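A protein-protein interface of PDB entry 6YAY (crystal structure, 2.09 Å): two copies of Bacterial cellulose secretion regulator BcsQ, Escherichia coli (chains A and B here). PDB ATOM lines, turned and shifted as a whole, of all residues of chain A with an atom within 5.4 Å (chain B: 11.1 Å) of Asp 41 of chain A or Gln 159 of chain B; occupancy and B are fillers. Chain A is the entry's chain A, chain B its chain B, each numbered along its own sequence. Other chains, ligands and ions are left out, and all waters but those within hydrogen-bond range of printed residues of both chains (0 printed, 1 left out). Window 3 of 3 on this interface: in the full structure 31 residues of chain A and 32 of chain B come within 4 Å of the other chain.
Among the printed residues, merely in contact across the chains: Gln 92 of chain A with Gln 160 of chain B (3.4 Å), Phe 52 of chain A with Gln 159 of chain B (3.5 Å), Leu 43 of chain A with Gln 159 of chain B (3.6 Å), Gln 92 of chain A with Ala 129 of chain B (3.6 Å), Leu 43 of chain A with Ile 155 of chain B (3.6 Å), Ile 89 of chain A with Ala 161 of chain B (3.7 Å), Gln 92 of chain A with Ala 161 of chain B (3.9 Å), Leu 43 of chain A with Asn 152 of chain B (3.9 Å), Phe 52 of chain A with His 158 of chain B (3.9 Å) and Leu 43 of chain A with Arg 156 of chain B (3.99 Å).
The side-chain carboxylate of Asp 41 of chain A is in salt-bridge range of the guanidinium group of Arg 156 of chain B (3.0 Å).
NE2 of Gln 159 of chain B lies within hydrogen-bond range of O of Asp 41 of chain A (3.0 Å).
The side-chain amide nitrogen of Gln 86 of chain A lies within hydrogen-bond range of the side-chain amide oxygen of Gln 159 of chain B (3.3 Å).
The side-chain amide nitrogen (NE2) of Gln 92 of chain A lies within hydrogen-bond range of the backbone carbonyl oxygen (O) of Gln 159 of chain B, at 3.2 Å.
No residue of chain B comes within 4 Å of Cys 39 of chain A.
No residue of chain B comes within 4 Å of Pro 40 of chain A.
Of chain B, only Arg 156 (3.0 Å) and Gln 159 (3.0 Å) come within 4 Å of Asp 41 of chain A.
Of the printed residues of chain B, Leu 43 of chain A touches Asn 152 (3.9 Å), Ile 155 (3.6 Å), Arg 156 (3.99 Å) and Gln 159 (3.6 Å).
Gly 11 of chain B touches none of the printed residues of chain A.
Of the printed residues of chain A, Ala 129 of chain B touches Gln 92 (3.6 Å).
Of the printed residues of chain A, Asn 152 of chain B touches Leu 43 (3.9 Å).
Of the printed residues of chain A, His 158 of chain B touches Phe 52 (3.9 Å).
Gln 159 of chain B touches just these residues of chain A: Asp 41 (3.0 Å), Leu 43 (3.6 Å), Phe 52 (3.5 Å), Gln 86 (3.3 Å) and Gln 92 (3.2 Å).
Of the printed residues of chain A, Gln 160 of chain B touches Gln 92 (3.4 Å).
Gln 191 of chain B touches none of the printed residues of chain A.
The nearest printed residue of chain A that does not touch Gln 159 of chain B is Arg 45 of chain A (4.6 Å).
The nearest printed residue of chain B that does not touch Leu 43 of chain A is Ala 151 of chain B (6.5 Å).
OD2 of Asp 37 of chain A sits at hydrogen-bond distance from N of Leu 43 of chain A.
The side-chain amide oxygen (OE1) of Gln 86 of chain A sits at hydrogen-bond distance from the side-chain amide nitrogen (ND2) of Asn 42 of chain A (3.0 Å).
The backbone carbonyl oxygen (O) of Phe 52 of chain A sits at hydrogen-bond distance from the guanidinium group (NH2) of Arg 45 of chain A.
The side-chain amide nitrogen (NE2) of Gln 86 of chain A lies close to the guanidinium group (NH2) of Arg 45 of chain A (3.2 Å).
O of Val 9 of chain B sits at hydrogen-bond distance from NE2 of Gln 160 of chain B, at 2.9 Å.
The side-chain amide oxygen (OD1) of Asn 152 of chain B is in hydrogen-bond range of the guanidinium group (NE) of Arg 156 of chain B, at 2.9 Å.
No position is printed for both chains.
Printed residues of chain B that touch a printed residue of chain A: Ala 129, Asn 152, Ile 155, Arg 156, His 158, Gln 159, Gln 160 and Ala 161.
Hydrophobic or aromatic side chains of chain B within 4 Å of the printed part of chain A: Ala 129, Ile 155 and Ala 161.
Hydrophobic or aromatic side chains of chain A within 4 Å of the printed part of chain B: Leu 43, Phe 52 and Ile 89.
Along chain A the printed residues that touch a printed residue of chain B span positions 41 to 92.
Among the printed residues, Asp or Glu carboxylates within 4 Å of a Lys or Arg side-chain nitrogen of the other chain: Asp 41 of chain A with Arg 156 of chain B.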
ATOM      1  N   ASP A  37      22.433  -7.147   4.185  1.00  0.00           N
ATOM      2  CA  ASP A  37      21.578  -5.968   4.140  1.00  0.00           C
ATOM      3  C   ASP A  37      22.457  -4.736   4.323  1.00  0.00           C
ATOM      4  O   ASP A  37      23.016  -4.518   5.403  1.00  0.00           O
ATOM      5  CB  ASP A  37      20.494  -6.035   5.211  1.00  0.00           C
ATOM      6  CG  ASP A  37      19.447  -4.950   5.044  1.00  0.00           C
ATOM      7  OD1 ASP A  37      19.496  -4.225   4.029  1.00  0.00           O
ATOM      8  OD2 ASP A  37      18.572  -4.822   5.924  1.00  0.00           O
ATOM      9  N   CYS A  39      21.085  -1.729   3.726  1.00  0.00           N
ATOM     10  CA  CYS A  39      20.107  -0.663   3.902  1.00  0.00           C
ATOM     11  C   CYS A  39      19.952  -0.338   5.380  1.00  0.00           C
ATOM     12  O   CYS A  39      19.716  -1.247   6.185  1.00  0.00           O
ATOM     13  CB  CYS A  39      18.762  -1.069   3.321  1.00  0.00           C
ATOM     14  SG  CYS A  39      18.808  -1.395   1.551  1.00  0.00           S
ATOM     15  N   PRO A  40      20.079   0.930   5.771  1.00  0.00           N
ATOM     16  CA  PRO A  40      19.910   1.281   7.191  1.00  0.00           C
ATOM     17  C   PRO A  40      18.516   0.997   7.716  1.00  0.00           C
ATOM     18  O   PRO A  40      18.334   0.923   8.939  1.00  0.00           O
ATOM     19  CB  PRO A  40      20.225   2.784   7.226  1.00  0.00           C
ATOM     20  CG  PRO A  40      20.931   3.073   5.933  1.00  0.00           C
ATOM     21  CD  PRO A  40      20.384   2.104   4.940  1.00  0.00           C
ATOM     22  N   ASP A  41      17.526   0.842   6.831  1.00  0.00           N
ATOM     23  CA  ASP A  41      16.196   0.424   7.260  1.00  0.00           C
ATOM     24  C   ASP A  41      16.229  -0.931   7.957  1.00  0.00           C
ATOM     25  O   ASP A  41      15.359  -1.222   8.788  1.00  0.00           O
ATOM     26  CB  ASP A  41      15.254   0.372   6.057  1.00  0.00           C
ATOM     27  CG  ASP A  41      15.457   1.534   5.102  1.00  0.00           C
ATOM     28  OD1 ASP A  41      15.410   2.702   5.549  1.00  0.00           O
ATOM     29  OD2 ASP A  41      15.669   1.274   3.898  1.00  0.00           O
ATOM     30  N   ASN A  42      17.210  -1.773   7.624  1.00  0.00           N
ATOM     31  CA  ASN A  42      17.415  -3.062   8.294  1.00  0.00           C
ATOM     32  C   ASN A  42      16.186  -3.960   8.152  1.00  0.00           C
ATOM     33  O   ASN A  42      15.754  -4.615   9.102  1.00  0.00           O
ATOM     34  CB  ASN A  42      17.786  -2.855   9.766  1.00  0.00           C
ATOM     35  CG  ASN A  42      18.327  -4.109  10.422  1.00  0.00           C
ATOM     36  OD1 ASN A  42      18.947  -4.955   9.771  1.00  0.00           O
ATOM     37  ND2 ASN A  42      18.091  -4.237  11.721  1.00  0.00           N
ATOM     38  N   LEU A  43      15.621  -3.997   6.945  1.00  0.00           N
ATOM     39  CA  LEU A  43      14.367  -4.695   6.699  1.00  0.00           C
ATOM     40  C   LEU A  43      14.547  -6.113   6.179  1.00  0.00           C
ATOM     41  O   LEU A  43      13.636  -6.931   6.338  1.00  0.00           O
ATOM     42  CB  LEU A  43      13.514  -3.906   5.698  1.00  0.00           C
ATOM     43  CG  LEU A  43      13.061  -2.523   6.167  1.00  0.00           C
ATOM     44  CD1 LEU A  43      12.281  -1.797   5.076  1.00  0.00           C
ATOM     45  CD2 LEU A  43      12.232  -2.648   7.431  1.00  0.00           C
ATOM     46  N   ARG A  45      16.250  -8.614   7.218  1.00  0.00           N
ATOM     47  CA  ARG A  45      16.212  -9.642   8.255  1.00  0.00           C
ATOM     48  C   ARG A  45      14.795 -10.139   8.521  1.00  0.00           C
ATOM     49  O   ARG A  45      14.609 -11.295   8.921  1.00  0.00           O
ATOM     50  CB  ARG A  45      16.822  -9.095   9.546  1.00  0.00           C
ATOM     51  CG  ARG A  45      15.965  -8.020  10.193  1.00  0.00           C
ATOM     52  CD  ARG A  45      16.698  -7.234  11.261  1.00  0.00           C
ATOM     53  NE  ARG A  45      15.867  -6.133  11.742  1.00  0.00           N
ATOM     54  CZ  ARG A  45      15.240  -6.120  12.914  1.00  0.00           C
ATOM     55  NH1 ARG A  45      15.359  -7.147  13.745  1.00  0.00           N
ATOM     56  NH2 ARG A  45      14.501  -5.075  13.260  1.00  0.00           N
ATOM     57  N   PHE A  52      12.004  -8.553  15.663  1.00  0.00           N
ATOM     58  CA  PHE A  52      12.173  -7.114  15.490  1.00  0.00           C
ATOM     59  C   PHE A  52      13.033  -6.514  16.593  1.00  0.00           C
ATOM     60  O   PHE A  52      13.773  -5.554  16.349  1.00  0.00           O
ATOM     61  CB  PHE A  52      10.814  -6.418  15.441  1.00  0.00           C
ATOM     62  CG  PHE A  52      10.907  -4.929  15.274  1.00  0.00           C
ATOM     63  CD1 PHE A  52      11.085  -4.371  14.019  1.00  0.00           C
ATOM     64  CD2 PHE A  52      10.830  -4.088  16.373  1.00  0.00           C
ATOM     65  CE1 PHE A  52      11.178  -3.001  13.862  1.00  0.00           C
ATOM     66  CE2 PHE A  52      10.925  -2.718  16.222  1.00  0.00           C
ATOM     67  CZ  PHE A  52      11.098  -2.174  14.965  1.00  0.00           C
ATOM     68  N   GLN A  86      19.878  -2.375  14.049  1.00  0.00           N
ATOM     69  CA  GLN A  86      18.933  -1.295  14.306  1.00  0.00           C
ATOM     70  C   GLN A  86      19.684  -0.029  14.697  1.00  0.00           C
ATOM     71  O   GLN A  86      20.472  -0.034  15.648  1.00  0.00           O
ATOM     72  CB  GLN A  86      17.947  -1.693  15.401  1.00  0.00           C
ATOM     73  CG  GLN A  86      16.947  -2.767  14.992  1.00  0.00           C
ATOM     74  CD  GLN A  86      15.947  -2.284  13.952  1.00  0.00           C
ATOM     75  OE1 GLN A  86      16.281  -2.118  12.777  1.00  0.00           O
ATOM     76  NE2 GLN A  86      14.709  -2.063  14.381  1.00  0.00           N
ATOM     77  N   LEU A  87      19.440   1.051  13.961  1.00  0.00           N
ATOM     78  CA  LEU A  87      19.972   2.359  14.308  1.00  0.00           C
ATOM     79  C   LEU A  87      19.018   3.066  15.258  1.00  0.00           C
ATOM     80  O   LEU A  87      17.797   2.988  15.104  1.00  0.00           O
ATOM     81  CB  LEU A  87      20.178   3.216  13.058  1.00  0.00           C
ATOM     82  CG  LEU A  87      21.261   2.817  12.059  1.00  0.00           C
ATOM     83  CD1 LEU A  87      21.219   3.758  10.866  1.00  0.00           C
ATOM     84  CD2 LEU A  87      22.633   2.840  12.716  1.00  0.00           C
ATOM     85  N   ILE A  89      17.149   6.387  16.813  1.00  0.00           N
ATOM     86  CA  ILE A  89      16.546   7.535  16.139  1.00  0.00           C
ATOM     87  C   ILE A  89      17.582   8.631  15.931  1.00  0.00           C
ATOM     88  O   ILE A  89      17.592   9.313  14.898  1.00  0.00           O
ATOM     89  CB  ILE A  89      15.331   8.042  16.938  1.00  0.00           C
ATOM     90  CG1 ILE A  89      14.286   6.934  17.073  1.00  0.00           C
ATOM     91  CG2 ILE A  89      14.729   9.275  16.282  1.00  0.00           C
ATOM     92  CD1 ILE A  89      13.077   7.341  17.882  1.00  0.00           C
ATOM     93  N   GLN A  92      19.738   7.620  12.986  1.00  0.00           N
ATOM     94  CA  GLN A  92      19.011   7.666  11.719  1.00  0.00           C
ATOM     95  C   GLN A  92      19.044   9.065  11.112  1.00  0.00           C
ATOM     96  O   GLN A  92      19.292   9.229   9.912  1.00  0.00           O
ATOM     97  CB  GLN A  92      17.561   7.210  11.920  1.00  0.00           C
ATOM     98  CG  GLN A  92      17.394   5.743  12.299  1.00  0.00           C
ATOM     99  CD  GLN A  92      15.938   5.353  12.507  1.00  0.00           C
ATOM    100  OE1 GLN A  92      15.026   6.060  12.076  1.00  0.00           O
ATOM    101  NE2 GLN A  92      15.716   4.225  13.171  1.00  0.00           N
ATOM    102  N   GLY B   8       7.466  11.074   1.871  1.00  0.00           N
ATOM    103  CA  GLY B   8       7.133   9.664   1.934  1.00  0.00           C
ATOM    104  C   GLY B   8       7.837   8.981   3.094  1.00  0.00           C
ATOM    105  O   GLY B   8       8.973   9.305   3.441  1.00  0.00           O
ATOM    106  N   VAL B   9       7.137   8.026   3.711  1.00  0.00           N
ATOM    107  CA  VAL B   9       7.776   7.177   4.711  1.00  0.00           C
ATOM    108  C   VAL B   9       8.819   6.284   4.047  1.00  0.00           C
ATOM    109  O   VAL B   9       9.804   5.881   4.681  1.00  0.00           O
ATOM    110  CB  VAL B   9       6.696   6.386   5.476  1.00  0.00           C
ATOM    111  CG1 VAL B   9       7.258   5.120   6.102  1.00  0.00           C
ATOM    112  CG2 VAL B   9       6.077   7.273   6.546  1.00  0.00           C
ATOM    113  N   ARG B  10       8.639   5.985   2.763  1.00  0.00           N
ATOM    114  CA  ARG B  10       9.677   5.420   1.916  1.00  0.00           C
ATOM    115  C   ARG B  10       9.515   6.015   0.525  1.00  0.00           C
ATOM    116  O   ARG B  10       8.559   6.751   0.252  1.00  0.00           O
ATOM    117  CB  ARG B  10       9.604   3.889   1.868  1.00  0.00           C
ATOM    118  CG  ARG B  10       8.423   3.377   1.080  1.00  0.00           C
ATOM    119  CD  ARG B  10       8.730   2.058   0.401  1.00  0.00           C
ATOM    120  NE  ARG B  10       7.645   1.672  -0.492  1.00  0.00           N
ATOM    121  CZ  ARG B  10       6.588   0.963  -0.114  1.00  0.00           C
ATOM    122  NH1 ARG B  10       6.482   0.555   1.143  1.00  0.00           N
ATOM    123  NH2 ARG B  10       5.643   0.662  -0.992  1.00  0.00           N
ATOM    124  N   GLY B  11      10.449   5.691  -0.366  1.00  0.00           N
ATOM    125  CA  GLY B  11      10.367   6.183  -1.725  1.00  0.00           C
ATOM    126  C   GLY B  11       9.286   5.490  -2.536  1.00  0.00           C
ATOM    127  O   GLY B  11       8.869   4.367  -2.254  1.00  0.00           O
ATOM    128  N   ARG B 127      13.101  11.361   0.698  1.00  0.00           N
ATOM    129  CA  ARG B 127      13.221  10.360   1.755  1.00  0.00           C
ATOM    130  C   ARG B 127      14.700  10.213   2.102  1.00  0.00           C
ATOM    131  O   ARG B 127      15.395   9.290   1.671  1.00  0.00           O
ATOM    132  CB  ARG B 127      12.594   9.040   1.310  1.00  0.00           C
ATOM    133  CG  ARG B 127      12.800   7.857   2.254  1.00  0.00           C
ATOM    134  CD  ARG B 127      11.885   7.896   3.466  1.00  0.00           C
ATOM    135  NE  ARG B 127      12.565   8.348   4.677  1.00  0.00           N
ATOM    136  CZ  ARG B 127      12.064   9.243   5.525  1.00  0.00           C
ATOM    137  NH1 ARG B 127      10.872   9.775   5.303  1.00  0.00           N
ATOM    138  NH2 ARG B 127      12.753   9.596   6.602  1.00  0.00           N
ATOM    139  N   ASP B 128      15.196  11.175   2.874  1.00  0.00           N
ATOM    140  CA  ASP B 128      16.529  11.084   3.453  1.00  0.00           C
ATOM    141  C   ASP B 128      16.558  11.918   4.726  1.00  0.00           C
ATOM    142  O   ASP B 128      15.536  12.457   5.166  1.00  0.00           O
ATOM    143  CB  ASP B 128      17.622  11.518   2.462  1.00  0.00           C
ATOM    144  CG  ASP B 128      17.476  12.961   1.996  1.00  0.00           C
ATOM    145  OD1 ASP B 128      17.511  13.887   2.835  1.00  0.00           O
ATOM    146  OD2 ASP B 128      17.358  13.171   0.771  1.00  0.00           O
ATOM    147  N   ALA B 129      17.743  12.020   5.316  1.00  0.00           N
ATOM    148  CA  ALA B 129      17.962  12.783   6.537  1.00  0.00           C
ATOM    149  C   ALA B 129      19.111  13.759   6.347  1.00  0.00           C
ATOM    150  O   ALA B 129      19.926  13.973   7.248  1.00  0.00           O
ATOM    151  CB  ALA B 129      18.224  11.857   7.721  1.00  0.00           C
ATOM    152  N   ALA B 151       3.356  -4.353   4.169  1.00  0.00           N
ATOM    153  CA  ALA B 151       4.187  -4.760   5.299  1.00  0.00           C
ATOM    154  C   ALA B 151       5.407  -3.860   5.459  1.00  0.00           C
ATOM    155  O   ALA B 151       5.849  -3.610   6.585  1.00  0.00           O
ATOM    156  CB  ALA B 151       4.611  -6.220   5.132  1.00  0.00           C
ATOM    157  N   ASN B 152       5.958  -3.364   4.350  1.00  0.00           N
ATOM    158  CA  ASN B 152       7.119  -2.479   4.413  1.00  0.00           C
ATOM    159  C   ASN B 152       6.804  -1.226   5.224  1.00  0.00           C
ATOM    160  O   ASN B 152       7.475  -0.928   6.219  1.00  0.00           O
ATOM    161  CB  ASN B 152       7.571  -2.127   2.991  1.00  0.00           C
ATOM    162  CG  ASN B 152       8.810  -1.236   2.955  1.00  0.00           C
ATOM    163  OD1 ASN B 152       8.926  -0.267   3.703  1.00  0.00           O
ATOM    164  ND2 ASN B 152       9.736  -1.559   2.061  1.00  0.00           N
ATOM    165  N   CYS B 153       5.785  -0.471   4.808  1.00  0.00           N
ATOM    166  CA  CYS B 153       5.420   0.738   5.540  1.00  0.00           C
ATOM    167  C   CYS B 153       4.988   0.420   6.965  1.00  0.00           C
ATOM    168  O   CYS B 153       5.274   1.188   7.891  1.00  0.00           O
ATOM    169  CB  CYS B 153       4.314   1.491   4.801  1.00  0.00           C
ATOM    170  SG  CYS B 153       4.861   2.351   3.302  1.00  0.00           S
ATOM    171  N   HIS B 154       4.302  -0.709   7.163  1.00  0.00           N
ATOM    172  CA  HIS B 154       3.862  -1.078   8.506  1.00  0.00           C
ATOM    173  C   HIS B 154       5.047  -1.231   9.453  1.00  0.00           C
ATOM    174  O   HIS B 154       4.976  -0.829  10.621  1.00  0.00           O
ATOM    175  CB  HIS B 154       3.042  -2.367   8.454  1.00  0.00           C
ATOM    176  CG  HIS B 154       2.560  -2.830   9.794  1.00  0.00           C
ATOM    177  ND1 HIS B 154       1.437  -2.312  10.402  1.00  0.00           N
ATOM    178  CD2 HIS B 154       3.051  -3.761  10.647  1.00  0.00           C
ATOM    179  CE1 HIS B 154       1.256  -2.903  11.569  1.00  0.00           C
ATOM    180  NE2 HIS B 154       2.222  -3.787  11.743  1.00  0.00           N
ATOM    181  N   ILE B 155       6.149  -1.803   8.966  1.00  0.00           N
ATOM    182  CA  ILE B 155       7.340  -1.928   9.798  1.00  0.00           C
ATOM    183  C   ILE B 155       7.960  -0.561  10.057  1.00  0.00           C
ATOM    184  O   ILE B 155       8.349  -0.244  11.189  1.00  0.00           O
ATOM    185  CB  ILE B 155       8.351  -2.885   9.145  1.00  0.00           C
ATOM    186  CG1 ILE B 155       7.759  -4.291   9.031  1.00  0.00           C
ATOM    187  CG2 ILE B 155       9.645  -2.903   9.944  1.00  0.00           C
ATOM    188  CD1 ILE B 155       8.398  -5.139   7.945  1.00  0.00           C
ATOM    189  N   ARG B 156       8.065   0.270   9.015  1.00  0.00           N
ATOM    190  CA  ARG B 156       8.742   1.557   9.153  1.00  0.00           C
ATOM    191  C   ARG B 156       8.061   2.450  10.182  1.00  0.00           C
ATOM    192  O   ARG B 156       8.737   3.206  10.887  1.00  0.00           O
ATOM    193  CB  ARG B 156       8.813   2.264   7.798  1.00  0.00           C
ATOM    194  CG  ARG B 156       9.799   1.646   6.812  1.00  0.00           C
ATOM    195  CD  ARG B 156       9.710   2.326   5.456  1.00  0.00           C
ATOM    196  NE  ARG B 156      10.706   1.828   4.511  1.00  0.00           N
ATOM    197  CZ  ARG B 156      11.918   2.353   4.364  1.00  0.00           C
ATOM    198  NH1 ARG B 156      12.289   3.386   5.108  1.00  0.00           N
ATOM    199  NH2 ARG B 156      12.763   1.847   3.476  1.00  0.00           N
ATOM    200  N   LEU B 157       6.732   2.368  10.295  1.00  0.00           N
ATOM    201  CA  LEU B 157       6.008   3.173  11.273  1.00  0.00           C
ATOM    202  C   LEU B 157       6.332   2.790  12.714  1.00  0.00           C
ATOM    203  O   LEU B 157       5.973   3.539  13.629  1.00  0.00           O
ATOM    204  CB  LEU B 157       4.502   3.056  11.038  1.00  0.00           C
ATOM    205  CG  LEU B 157       3.976   3.643   9.725  1.00  0.00           C
ATOM    206  CD1 LEU B 157       2.459   3.502   9.632  1.00  0.00           C
ATOM    207  CD2 LEU B 157       4.389   5.099   9.591  1.00  0.00           C
ATOM    208  N   HIS B 158       6.992   1.657  12.937  1.00  0.00           N
ATOM    209  CA  HIS B 158       7.392   1.235  14.271  1.00  0.00           C
ATOM    210  C   HIS B 158       8.861   1.505  14.568  1.00  0.00           C
ATOM    211  O   HIS B 158       9.304   1.252  15.693  1.00  0.00           O
ATOM    212  CB  HIS B 158       7.103  -0.258  14.468  1.00  0.00           C
ATOM    213  CG  HIS B 158       5.645  -0.596  14.479  1.00  0.00           C
ATOM    214  ND1 HIS B 158       4.880  -0.631  13.333  1.00  0.00           N
ATOM    215  CD2 HIS B 158       4.812  -0.912  15.498  1.00  0.00           C
ATOM    216  CE1 HIS B 158       3.639  -0.956  13.646  1.00  0.00           C
ATOM    217  NE2 HIS B 158       3.570  -1.134  14.953  1.00  0.00           N
ATOM    218  N   GLN B 159       9.627   2.010  13.602  1.00  0.00           N
ATOM    219  CA  GLN B 159      11.062   2.158  13.826  1.00  0.00           C
ATOM    220  C   GLN B 159      11.653   3.490  13.378  1.00  0.00           C
ATOM    221  O   GLN B 159      12.639   3.924  13.983  1.00  0.00           O
ATOM    222  CB  GLN B 159      11.826   1.020  13.140  1.00  0.00           C
ATOM    223  CG  GLN B 159      11.749   1.023  11.628  1.00  0.00           C
ATOM    224  CD  GLN B 159      12.587  -0.081  11.018  1.00  0.00           C
ATOM    225  OE1 GLN B 159      13.016  -1.000  11.714  1.00  0.00           O
ATOM    226  NE2 GLN B 159      12.832   0.009   9.716  1.00  0.00           N
ATOM    227  N   GLN B 160      11.115   4.158  12.362  1.00  0.00           N
ATOM    228  CA  GLN B 160      11.695   5.411  11.906  1.00  0.00           C
ATOM    229  C   GLN B 160      10.859   6.588  12.387  1.00  0.00           C
ATOM    230  O   GLN B 160       9.636   6.500  12.516  1.00  0.00           O
ATOM    231  CB  GLN B 160      11.837   5.443  10.381  1.00  0.00           C
ATOM    232  CG  GLN B 160      10.577   5.763   9.611  1.00  0.00           C
ATOM    233  CD  GLN B 160      10.774   5.640   8.113  1.00  0.00           C
ATOM    234  OE1 GLN B 160      11.308   4.643   7.628  1.00  0.00           O
ATOM    235  NE2 GLN B 160      10.344   6.655   7.372  1.00  0.00           N
ATOM    236  N   ALA B 161      11.542   7.690  12.672  1.00  0.00           N
ATOM    237  CA  ALA B 161      10.882   8.874  13.196  1.00  0.00           C
ATOM    238  C   ALA B 161      10.250   9.680  12.072  1.00  0.00           C
ATOM    239  O   ALA B 161      10.750   9.722  10.944  1.00  0.00           O
ATOM    240  CB  ALA B 161      11.873   9.746  13.967  1.00  0.00           C
ATOM    241  N   LEU B 162       9.133  10.315  12.393  1.00  0.00           N
ATOM    242  CA  LEU B 162       8.452  11.242  11.510  1.00  0.00           C
ATOM    243  C   LEU B 162       8.532  12.655  12.075  1.00  0.00           C
ATOM    244  O   LEU B 162       8.855  12.845  13.253  1.00  0.00           O
ATOM    245  CB  LEU B 162       6.982  10.836  11.331  1.00  0.00           C
ATOM    246  CG  LEU B 162       6.728   9.437  10.771  1.00  0.00           C
ATOM    247  CD1 LEU B 162       5.264   9.281  10.391  1.00  0.00           C
ATOM    248  CD2 LEU B 162       7.640   9.152   9.582  1.00  0.00           C
ATOM    249  N   PRO B 163       8.278  13.675  11.258  1.00  0.00           N
ATOM    250  CA  PRO B 163       8.191  15.034  11.802  1.00  0.00           C
ATOM    251  C   PRO B 163       7.106  15.117  12.865  1.00  0.00           C
ATOM    252  O   PRO B 163       6.056  14.481  12.757  1.00  0.00           O
ATOM    253  CB  PRO B 163       7.851  15.887  10.576  1.00  0.00           C
ATOM    254  CG  PRO B 163       8.386  15.109   9.425  1.00  0.00           C
ATOM    255  CD  PRO B 163       8.204  13.665   9.785  1.00  0.00           C
ATOM    256  N   ILE B 168      -0.576  10.948   8.701  1.00  0.00           N
ATOM    257  CA  ILE B 168      -0.243   9.884   7.763  1.00  0.00           C
ATOM    258  C   ILE B 168      -1.319   9.811   6.688  1.00  0.00           C
ATOM    259  O   ILE B 168      -2.514   9.743   6.998  1.00  0.00           O
ATOM    260  CB  ILE B 168      -0.100   8.539   8.496  1.00  0.00           C
ATOM    261  CG1 ILE B 168       1.003   8.633   9.551  1.00  0.00           C
ATOM    262  CG2 ILE B 168       0.180   7.420   7.512  1.00  0.00           C
ATOM    263  CD1 ILE B 168       1.031   7.468  10.509  1.00  0.00           C
ATOM    264  N   TRP B 187      -4.598  -0.646  11.189  1.00  0.00           N
ATOM    265  CA  TRP B 187      -4.259   0.770  11.313  1.00  0.00           C
ATOM    266  C   TRP B 187      -5.450   1.587  11.793  1.00  0.00           C
ATOM    267  O   TRP B 187      -5.284   2.551  12.550  1.00  0.00           O
ATOM    268  CB  TRP B 187      -3.751   1.315   9.978  1.00  0.00           C
ATOM    269  CG  TRP B 187      -2.374   0.857   9.608  1.00  0.00           C
ATOM    270  CD1 TRP B 187      -1.597  -0.039  10.284  1.00  0.00           C
ATOM    271  CD2 TRP B 187      -1.609   1.276   8.471  1.00  0.00           C
ATOM    272  NE1 TRP B 187      -0.396  -0.204   9.637  1.00  0.00           N
ATOM    273  CE2 TRP B 187      -0.377   0.593   8.523  1.00  0.00           C
ATOM    274  CE3 TRP B 187      -1.845   2.164   7.417  1.00  0.00           C
ATOM    275  CZ2 TRP B 187       0.616   0.769   7.559  1.00  0.00           C
ATOM    276  CZ3 TRP B 187      -0.858   2.337   6.462  1.00  0.00           C
ATOM    277  CH2 TRP B 187       0.357   1.642   6.539  1.00  0.00           C
ATOM    278  N   GLN B 191      -3.276   3.256  14.660  1.00  0.00           N
ATOM    279  CA  GLN B 191      -2.518   4.418  14.198  1.00  0.00           C
ATOM    280  C   GLN B 191      -3.285   5.683  14.564  1.00  0.00           C
ATOM    281  O   GLN B 191      -4.246   6.060  13.889  1.00  0.00           O
ATOM    282  CB  GLN B 191      -2.271   4.330  12.697  1.00  0.00           C
ATOM    283  CG  GLN B 191      -1.442   3.125  12.273  1.00  0.00           C
ATOM    284  CD  GLN B 191       0.021   3.247  12.664  1.00  0.00           C
ATOM    285  OE1 GLN B 191       0.518   4.342  12.930  1.00  0.00           O
ATOM    286  NE2 GLN B 191       0.717   2.118  12.698  1.00  0.00           N
